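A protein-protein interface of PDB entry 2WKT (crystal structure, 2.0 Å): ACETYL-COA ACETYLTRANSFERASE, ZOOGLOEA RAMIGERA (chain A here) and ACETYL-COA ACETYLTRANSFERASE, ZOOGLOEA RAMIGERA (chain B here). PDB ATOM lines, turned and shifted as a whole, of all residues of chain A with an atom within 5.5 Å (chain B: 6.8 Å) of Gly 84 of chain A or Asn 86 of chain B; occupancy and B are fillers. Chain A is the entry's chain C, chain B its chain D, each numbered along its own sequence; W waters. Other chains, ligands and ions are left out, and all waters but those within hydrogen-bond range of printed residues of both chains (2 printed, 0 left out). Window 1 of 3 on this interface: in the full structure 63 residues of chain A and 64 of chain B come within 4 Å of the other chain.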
ATOM      1  N   LEU A  54      -6.814   9.875   4.032  1.00  0.00           N
ATOM      2  CA  LEU A  54      -7.460  11.003   4.699  1.00  0.00           C
ATOM      3  C   LEU A  54      -6.876  11.300   6.076  1.00  0.00           C
ATOM      4  O   LEU A  54      -6.844  10.439   6.953  1.00  0.00           O
ATOM      5  CB  LEU A  54      -8.979  10.802   4.775  1.00  0.00           C
ATOM      6  CG  LEU A  54      -9.682  10.912   3.408  1.00  0.00           C
ATOM      7  CD1 LEU A  54     -11.191  10.627   3.504  1.00  0.00           C
ATOM      8  CD2 LEU A  54      -9.429  12.258   2.775  1.00  0.00           C
ATOM      9  N   GLY A  55      -6.402  12.533   6.234  1.00  0.00           N
ATOM     10  CA  GLY A  55      -6.003  13.056   7.517  1.00  0.00           C
ATOM     11  C   GLY A  55      -7.229  13.280   8.397  1.00  0.00           C
ATOM     12  O   GLY A  55      -8.273  13.743   7.941  1.00  0.00           O
ATOM     13  N   ASN A  65     -12.205   2.943  10.794  1.00  0.00           N
ATOM     14  CA  ASN A  65     -11.537   3.619   9.677  1.00  0.00           C
ATOM     15  C   ASN A  65     -12.460   4.504   8.818  1.00  0.00           C
ATOM     16  O   ASN A  65     -12.813   4.135   7.709  1.00  0.00           O
ATOM     17  CB  ASN A  65     -10.804   2.584   8.805  1.00  0.00           C
ATOM     18  CG  ASN A  65      -9.868   3.222   7.788  1.00  0.00           C
ATOM     19  OD1 ASN A  65      -9.529   4.400   7.889  1.00  0.00           O
ATOM     20  ND2 ASN A  65      -9.442   2.438   6.799  1.00  0.00           N
ATOM     21  N   PRO A  66     -12.846   5.682   9.339  1.00  0.00           N
ATOM     22  CA  PRO A  66     -13.753   6.617   8.648  1.00  0.00           C
ATOM     23  C   PRO A  66     -13.309   6.880   7.202  1.00  0.00           C
ATOM     24  O   PRO A  66     -14.133   7.101   6.314  1.00  0.00           O
ATOM     25  CB  PRO A  66     -13.611   7.900   9.457  1.00  0.00           C
ATOM     26  CG  PRO A  66     -13.227   7.434  10.831  1.00  0.00           C
ATOM     27  CD  PRO A  66     -12.341   6.239  10.609  1.00  0.00           C
ATOM     28  N   ALA A  67     -12.007   6.861   6.985  1.00  0.00           N
ATOM     29  CA  ALA A  67     -11.453   6.966   5.633  1.00  0.00           C
ATOM     30  C   ALA A  67     -11.973   5.911   4.634  1.00  0.00           C
ATOM     31  O   ALA A  67     -12.309   6.243   3.482  1.00  0.00           O
ATOM     32  CB  ALA A  67      -9.934   6.932   5.708  1.00  0.00           C
ATOM     33  N   ALA A  82      -7.826   2.060   1.772  1.00  0.00           N
ATOM     34  CA  ALA A  82      -8.033   3.362   2.375  1.00  0.00           C
ATOM     35  C   ALA A  82      -7.567   3.350   3.831  1.00  0.00           C
ATOM     36  O   ALA A  82      -7.659   2.335   4.515  1.00  0.00           O
ATOM     37  CB  ALA A  82      -9.504   3.750   2.298  1.00  0.00           C
ATOM     38  N   TRP A  83      -7.069   4.490   4.294  1.00  0.00           N
ATOM     39  CA  TRP A  83      -6.589   4.614   5.648  1.00  0.00           C
ATOM     40  C   TRP A  83      -6.557   6.078   6.067  1.00  0.00           C
ATOM     41  O   TRP A  83      -6.504   6.979   5.224  1.00  0.00           O
ATOM     42  CB  TRP A  83      -5.197   3.983   5.814  1.00  0.00           C
ATOM     43  CG  TRP A  83      -4.131   4.390   4.774  1.00  0.00           C
ATOM     44  CD1 TRP A  83      -4.016   3.926   3.498  1.00  0.00           C
ATOM     45  CD2 TRP A  83      -3.025   5.301   4.967  1.00  0.00           C
ATOM     46  NE1 TRP A  83      -2.921   4.501   2.869  1.00  0.00           N
ATOM     47  CE2 TRP A  83      -2.297   5.345   3.753  1.00  0.00           C
ATOM     48  CE3 TRP A  83      -2.586   6.084   6.047  1.00  0.00           C
ATOM     49  CZ2 TRP A  83      -1.164   6.148   3.583  1.00  0.00           C
ATOM     50  CZ3 TRP A  83      -1.454   6.877   5.880  1.00  0.00           C
ATOM     51  CH2 TRP A  83      -0.749   6.898   4.655  1.00  0.00           C
ATOM     52  N   GLY A  84      -6.606   6.307   7.374  1.00  0.00           N
ATOM     53  CA  GLY A  84      -6.406   7.636   7.910  1.00  0.00           C
ATOM     54  C   GLY A  84      -5.047   7.806   8.567  1.00  0.00           C
ATOM     55  O   GLY A  84      -4.346   6.838   8.877  1.00  0.00           O
ATOM     56  N   MET A  85      -4.673   9.053   8.801  1.00  0.00           N
ATOM     57  CA  MET A  85      -3.417   9.350   9.480  1.00  0.00           C
ATOM     58  C   MET A  85      -3.512  10.660  10.226  1.00  0.00           C
ATOM     59  O   MET A  85      -4.305  11.540   9.886  1.00  0.00           O
ATOM     60  CB  MET A  85      -2.213   9.373   8.500  1.00  0.00           C
ATOM     61  CG  MET A  85      -2.369  10.263   7.287  1.00  0.00           C
ATOM     62  SD  MET A  85      -2.259  12.044   7.590  1.00  0.00           S
ATOM     63  CE  MET A  85      -0.739  12.162   8.522  1.00  0.00           C
ATOM     64  N   ASN A  86      -2.681  10.780  11.247  1.00  0.00           N
ATOM     65  CA  ASN A  86      -2.754  11.915  12.135  1.00  0.00           C
ATOM     66  C   ASN A  86      -1.394  12.569  12.295  1.00  0.00           C
ATOM     67  O   ASN A  86      -0.517  12.020  12.943  1.00  0.00           O
ATOM     68  CB  ASN A  86      -3.319  11.463  13.490  1.00  0.00           C
ATOM     69  CG  ASN A  86      -3.338  12.562  14.516  1.00  0.00           C
ATOM     70  OD1 ASN A  86      -2.979  13.705  14.227  1.00  0.00           O
ATOM     71  ND2 ASN A  86      -3.768  12.225  15.738  1.00  0.00           N
ATOM     72  N   LEU B  54       3.810   5.637  13.853  1.00  0.00           N
ATOM     73  CA  LEU B  54       3.180   4.565  14.601  1.00  0.00           C
ATOM     74  C   LEU B  54       1.713   4.349  14.259  1.00  0.00           C
ATOM     75  O   LEU B  54       0.893   5.272  14.335  1.00  0.00           O
ATOM     76  CB  LEU B  54       3.386   4.752  16.110  1.00  0.00           C
ATOM     77  CG  LEU B  54       4.853   4.566  16.522  1.00  0.00           C
ATOM     78  CD1 LEU B  54       5.111   5.150  17.917  1.00  0.00           C
ATOM     79  CD2 LEU B  54       5.320   3.075  16.413  1.00  0.00           C
ATOM     80  N   GLY B  55       1.408   3.117  13.861  1.00  0.00           N
ATOM     81  CA  GLY B  55       0.039   2.690  13.656  1.00  0.00           C
ATOM     82  C   GLY B  55      -0.647   2.590  14.999  1.00  0.00           C
ATOM     83  O   GLY B  55      -0.042   2.159  15.984  1.00  0.00           O
ATOM     84  N   GLN B  56      -1.909   3.005  15.043  1.00  0.00           N
ATOM     85  CA  GLN B  56      -2.681   2.997  16.272  1.00  0.00           C
ATOM     86  C   GLN B  56      -4.135   3.305  15.944  1.00  0.00           C
ATOM     87  O   GLN B  56      -4.451   4.326  15.336  1.00  0.00           O
ATOM     88  CB  GLN B  56      -2.136   4.001  17.275  1.00  0.00           C
ATOM     89  CG  GLN B  56      -3.025   4.165  18.512  1.00  0.00           C
ATOM     90  CD  GLN B  56      -2.438   5.144  19.486  1.00  0.00           C
ATOM     91  OE1 GLN B  56      -1.669   6.037  19.099  1.00  0.00           O
ATOM     92  NE2 GLN B  56      -2.767   4.983  20.761  1.00  0.00           N
ATOM     93  N   VAL B  57      -5.006   2.386  16.334  1.00  0.00           N
ATOM     94  CA  VAL B  57      -6.411   2.426  15.969  1.00  0.00           C
ATOM     95  C   VAL B  57      -7.231   3.080  17.073  1.00  0.00           C
ATOM     96  O   VAL B  57      -8.288   3.660  16.812  1.00  0.00           O
ATOM     97  CB  VAL B  57      -6.935   0.987  15.768  1.00  0.00           C
ATOM     98  CG1 VAL B  57      -8.384   0.981  15.244  1.00  0.00           C
ATOM     99  CG2 VAL B  57      -6.023   0.239  14.842  1.00  0.00           C
ATOM    100  N   LEU B  58      -6.747   2.992  18.308  1.00  0.00           N
ATOM    101  CA  LEU B  58      -7.555   3.438  19.454  1.00  0.00           C
ATOM    102  C   LEU B  58      -6.826   4.451  20.349  1.00  0.00           C
ATOM    103  O   LEU B  58      -6.415   4.124  21.458  1.00  0.00           O
ATOM    104  CB  LEU B  58      -8.009   2.218  20.258  1.00  0.00           C
ATOM    105  CG  LEU B  58      -8.617   1.105  19.386  1.00  0.00           C
ATOM    106  CD1 LEU B  58      -8.733  -0.220  20.126  1.00  0.00           C
ATOM    107  CD2 LEU B  58      -9.968   1.526  18.814  1.00  0.00           C
ATOM    108  N   PRO B  59      -6.666   5.690  19.855  1.00  0.00           N
ATOM    109  CA  PRO B  59      -5.976   6.808  20.515  1.00  0.00           C
ATOM    110  C   PRO B  59      -6.904   7.675  21.396  1.00  0.00           C
ATOM    111  O   PRO B  59      -6.429   8.556  22.120  1.00  0.00           O
ATOM    112  CB  PRO B  59      -5.508   7.642  19.331  1.00  0.00           C
ATOM    113  CG  PRO B  59      -6.597   7.459  18.309  1.00  0.00           C
ATOM    114  CD  PRO B  59      -7.196   6.082  18.537  1.00  0.00           C
ATOM    115  N   TRP B  83       4.044  10.971  13.555  1.00  0.00           N
ATOM    116  CA  TRP B  83       2.618  10.862  13.234  1.00  0.00           C
ATOM    117  C   TRP B  83       2.099   9.441  13.404  1.00  0.00           C
ATOM    118  O   TRP B  83       2.871   8.498  13.329  1.00  0.00           O
ATOM    119  CB  TRP B  83       2.318  11.353  11.809  1.00  0.00           C
ATOM    120  CG  TRP B  83       3.151  10.762  10.697  1.00  0.00           C
ATOM    121  CD1 TRP B  83       4.452  11.070  10.395  1.00  0.00           C
ATOM    122  CD2 TRP B  83       2.718   9.830   9.684  1.00  0.00           C
ATOM    123  NE1 TRP B  83       4.866  10.360   9.284  1.00  0.00           N
ATOM    124  CE2 TRP B  83       3.820   9.599   8.826  1.00  0.00           C
ATOM    125  CE3 TRP B  83       1.515   9.162   9.428  1.00  0.00           C
ATOM    126  CZ2 TRP B  83       3.754   8.728   7.732  1.00  0.00           C
ATOM    127  CZ3 TRP B  83       1.447   8.301   8.341  1.00  0.00           C
ATOM    128  CH2 TRP B  83       2.565   8.088   7.506  1.00  0.00           C
ATOM    129  N   GLY B  84       0.794   9.303  13.651  1.00  0.00           N
ATOM    130  CA  GLY B  84       0.148   7.998  13.702  1.00  0.00           C
ATOM    131  C   GLY B  84      -0.677   7.729  12.465  1.00  0.00           C
ATOM    132  O   GLY B  84      -1.054   8.664  11.745  1.00  0.00           O
ATOM    133  N   MET B  85      -0.949   6.451  12.203  1.00  0.00           N
ATOM    134  CA  MET B  85      -1.822   6.062  11.098  1.00  0.00           C
ATOM    135  C   MET B  85      -2.673   4.846  11.422  1.00  0.00           C
ATOM    136  O   MET B  85      -2.309   4.006  12.259  1.00  0.00           O
ATOM    137  CB  MET B  85      -1.050   5.876   9.782  1.00  0.00           C
ATOM    138  CG  MET B  85       0.077   4.847   9.818  1.00  0.00           C
ATOM    139  SD  MET B  85      -0.503   3.148   9.706  1.00  0.00           S
ATOM    140  CE  MET B  85      -1.431   3.210   8.178  1.00  0.00           C
ATOM    141  N   ASN B  86      -3.814   4.769  10.746  1.00  0.00           N
ATOM    142  CA  ASN B  86      -4.823   3.751  11.011  1.00  0.00           C
ATOM    143  C   ASN B  86      -5.229   3.099   9.696  1.00  0.00           C
ATOM    144  O   ASN B  86      -5.837   3.740   8.836  1.00  0.00           O
ATOM    145  CB  ASN B  86      -6.028   4.402  11.723  1.00  0.00           C
ATOM    146  CG  ASN B  86      -7.168   3.415  12.037  1.00  0.00           C
ATOM    147  OD1 ASN B  86      -7.082   2.224  11.764  1.00  0.00           O
ATOM    148  ND2 ASN B  86      -8.252   3.937  12.611  1.00  0.00           N
ATOM    149  N   GLN B  87      -4.815   1.849   9.514  1.00  0.00           N
ATOM    150  CA  GLN B  87      -5.406   0.964   8.509  1.00  0.00           C
ATOM    151  C   GLN B  87      -5.819  -0.282   9.287  1.00  0.00           C
ATOM    152  O   GLN B  87      -5.528  -1.425   8.910  1.00  0.00           O
ATOM    153  CB  GLN B  87      -4.426   0.634   7.356  1.00  0.00           C
ATOM    154  CG  GLN B  87      -5.131   0.079   6.098  1.00  0.00           C
ATOM    155  CD  GLN B  87      -4.182  -0.280   4.949  1.00  0.00           C
ATOM    156  OE1 GLN B  87      -2.966  -0.058   5.017  1.00  0.00           O
ATOM    157  NE2 GLN B  87      -4.747  -0.838   3.876  1.00  0.00           N
ATOM    158  N   LEU B  88      -6.470  -0.035  10.421  1.00  0.00           N
ATOM    159  CA  LEU B  88      -6.896  -1.105  11.303  1.00  0.00           C
ATOM    160  C   LEU B  88      -5.793  -2.138  11.546  1.00  0.00           C
ATOM    161  O   LEU B  88      -4.647  -1.788  11.821  1.00  0.00           O
ATOM    162  CB  LEU B  88      -8.144  -1.780  10.741  1.00  0.00           C
ATOM    163  CG  LEU B  88      -9.394  -0.903  10.643  1.00  0.00           C
ATOM    164  CD1 LEU B  88     -10.595  -1.785  10.403  1.00  0.00           C
ATOM    165  CD2 LEU B  88      -9.594  -0.070  11.906  1.00  0.00           C
ATOM    166  N   CSO B  89      -6.133  -3.417  11.454  1.00  0.00           N
ATOM    167  CA  CSO B  89      -5.164  -4.444  11.805  1.00  0.00           C
ATOM    168  CB  CSO B  89      -5.831  -5.812  11.948  1.00  0.00           C
ATOM    169  SG  CSO B  89      -7.579  -5.596  12.371  1.00  0.00           S
ATOM    170  C   CSO B  89      -3.938  -4.483  10.884  1.00  0.00           C
ATOM    171  O   CSO B  89      -2.963  -5.172  11.177  1.00  0.00           O
ATOM    172  OD  CSO B  89      -8.629  -6.486  11.253  1.00  0.00           O
ATOM    173  N   GLY B  90      -3.979  -3.722   9.793  1.00  0.00           N
ATOM    174  CA  GLY B  90      -2.843  -3.637   8.889  1.00  0.00           C
ATOM    175  C   GLY B  90      -1.847  -2.560   9.290  1.00  0.00           C
ATOM    176  O   GLY B  90      -0.696  -2.532   8.800  1.00  0.00           O
ATOM    177  N   SER B  91      -2.285  -1.681  10.189  1.00  0.00           N
ATOM    178  CA  SER B  91      -1.518  -0.485  10.569  1.00  0.00           C
ATOM    179  C   SER B  91      -0.061  -0.787  10.874  1.00  0.00           C
ATOM    180  O   SER B  91       0.845  -0.196  10.278  1.00  0.00           O
ATOM    181  CB  SER B  91      -2.143   0.196  11.796  1.00  0.00           C
ATOM    182  OG  SER B  91      -3.424   0.736  11.509  1.00  0.00           O
ATOM    183  N   GLU B 117      -0.793  -0.222  20.637  1.00  0.00           N
ATOM    184  CA  GLU B 117      -2.216  -0.270  20.915  1.00  0.00           C
ATOM    185  C   GLU B 117      -2.431  -0.667  22.360  1.00  0.00           C
ATOM    186  O   GLU B 117      -1.746  -1.563  22.876  1.00  0.00           O
ATOM    187  CB  GLU B 117      -2.898  -1.287  19.987  1.00  0.00           C
ATOM    188  CG  GLU B 117      -4.384  -1.062  19.752  1.00  0.00           C
ATOM    189  CD  GLU B 117      -4.682   0.171  18.905  1.00  0.00           C
ATOM    190  OE1 GLU B 117      -4.956   1.246  19.485  1.00  0.00           O
ATOM    191  OE2 GLU B 117      -4.665   0.065  17.658  1.00  0.00           O
ATOM    192  N   ASP B 146     -14.995   1.451  17.081  1.00  0.00           N
ATOM    193  CA  ASP B 146     -13.967   1.922  16.149  1.00  0.00           C
ATOM    194  C   ASP B 146     -12.943   0.839  15.826  1.00  0.00           C
ATOM    195  O   ASP B 146     -12.183   0.943  14.849  1.00  0.00           O
ATOM    196  CB  ASP B 146     -13.269   3.168  16.717  1.00  0.00           C
ATOM    197  CG  ASP B 146     -14.259   4.255  17.157  1.00  0.00           C
ATOM    198  OD1 ASP B 146     -15.359   4.337  16.581  1.00  0.00           O
ATOM    199  OD2 ASP B 146     -13.928   5.051  18.062  1.00  0.00           O
ATOM    200  N   ILE B 350      -4.423  -4.748  17.957  1.00  0.00           N
ATOM    201  CA  ILE B 350      -4.739  -4.242  16.628  1.00  0.00           C
ATOM    202  C   ILE B 350      -3.614  -3.411  16.006  1.00  0.00           C
ATOM    203  O   ILE B 350      -2.948  -3.874  15.088  1.00  0.00           O
ATOM    204  CB  ILE B 350      -6.056  -3.421  16.621  1.00  0.00           C
ATOM    205  CG1 ILE B 350      -7.220  -4.245  17.165  1.00  0.00           C
ATOM    206  CG2 ILE B 350      -6.400  -2.972  15.216  1.00  0.00           C
ATOM    207  CD1 ILE B 350      -8.538  -3.462  17.216  1.00  0.00           C
HETATM  208  O   HOH W   1      -4.403   8.735  12.752  1.00  0.00           O
HETATM  209  O   HOH W   2     -10.921   3.215  13.370  1.00  0.00           O
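Water W2 lies within hydrogen-bond range of the side-chain amide nitrogen (ND2) of Asn 86 of chain B (2.9 Å), the backbone NH (N) of Asn 65 of chain A (2.9 Å) and the backbone carbonyl oxygen (O) of Asp 146 of chain B (3.0 Å). Water W1 lies within hydrogen-bond range of the backbone NH (N) of Asn 86 of chain A and the backbone carbonyl oxygen (O) of Gly 84 of chain B.
The backbone carbonyl oxygen (O) of Gly 84 of chain B is in hydrogen-bond range of the backbone NH (N) of Asn 86 of chain A. The backbone NH (N) of Asn 86 of chain B is in hydrogen-bond range of the backbone carbonyl oxygen (O) of Gly 84 of chain A (2.8 Å).
Printed residues of chain A that touch a printed residue of chain B: Asn 65, Ala 82, Trp 83, Gly 84, Met 85 and Asn 86. Hydrophobic or aromatic side chains of chain A that line the printed part of chain B: Trp 83 and Met 85. Hydrophobic or aromatic side chains of chain B within 4 Å of the printed part of chain A: Trp 83 and Met 85.
Of the printed residues of chain B, Gly 84 of chain A touches Met 85 (3.5 Å) and Asn 86 (2.8 Å). Asn 86 of chain B touches just these residues of chain A: Asn 65 (3.9 Å), Trp 83 (3.1 Å) and Gly 84 (2.8 Å). Of the printed residues of chain B, Ala 82 of chain A touches Gln 87. Printed residues of chain B within 4 Å of Met 85 of chain A: Trp 83 (3.8 Å), Gly 84 (3.3 Å) and Met 85 (3.9 Å). Printed residues of chain A within 4 Å of Gly 84 of chain B: Met 85 (3.3 Å) and Asn 86 (2.7 Å). Of the printed residues of chain A, Gln 87 of chain B touches Ala 82 (3.7 Å) and Trp 83 (3.8 Å). The nearest printed residue of chain A that does not touch Gly 84 of chain B is Gly 84 of chain A (4.7 Å).
The backbone NH of Met 85 of chain B lies within hydrogen-bond range of the backbone carbonyl oxygen of Leu 54 of chain B (3.1 Å). The backbone carbonyl oxygen (O) of Met 85 of chain B sits at hydrogen-bond distance from the backbone NH (N) of Gln 56 of chain B. The side-chain amide oxygen of Asn 86 of chain B lies within hydrogen-bond range of the backbone NH of Leu 88 of chain B, 2.7 Å away. N of Leu 54 of chain A lies within hydrogen-bond range of O of Trp 83 of chain A (3.1 Å). N of Met 85 of chain A lies within hydrogen-bond range of O of Leu 54 of chain A. The backbone carbonyl oxygen (O) of Ala 82 of chain A is in hydrogen-bond range of the side-chain amide nitrogen (ND2) of Asn 65 of chain A.
Among the printed residues, pairs that only touch across the chains: Trp 83 of chain A with Asn 86 of chain B, Asn 86 of chain A with Trp 83 of chain B, Met 85 of chain A with Gly 84 of chain B, Gly 84 of chain A with Met 85 of chain B, Ala 82 of chain A with Gln 87 of chain B, Trp 83 of chain A with Met 85 of chain B, Trp 83 of chain A with Gln 87 of chain B, Met 85 of chain A with Trp 83 of chain B, Asn 65 of chain A with Asn 86 of chain B and Met 85 of chain A with Met 85 of chain B.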
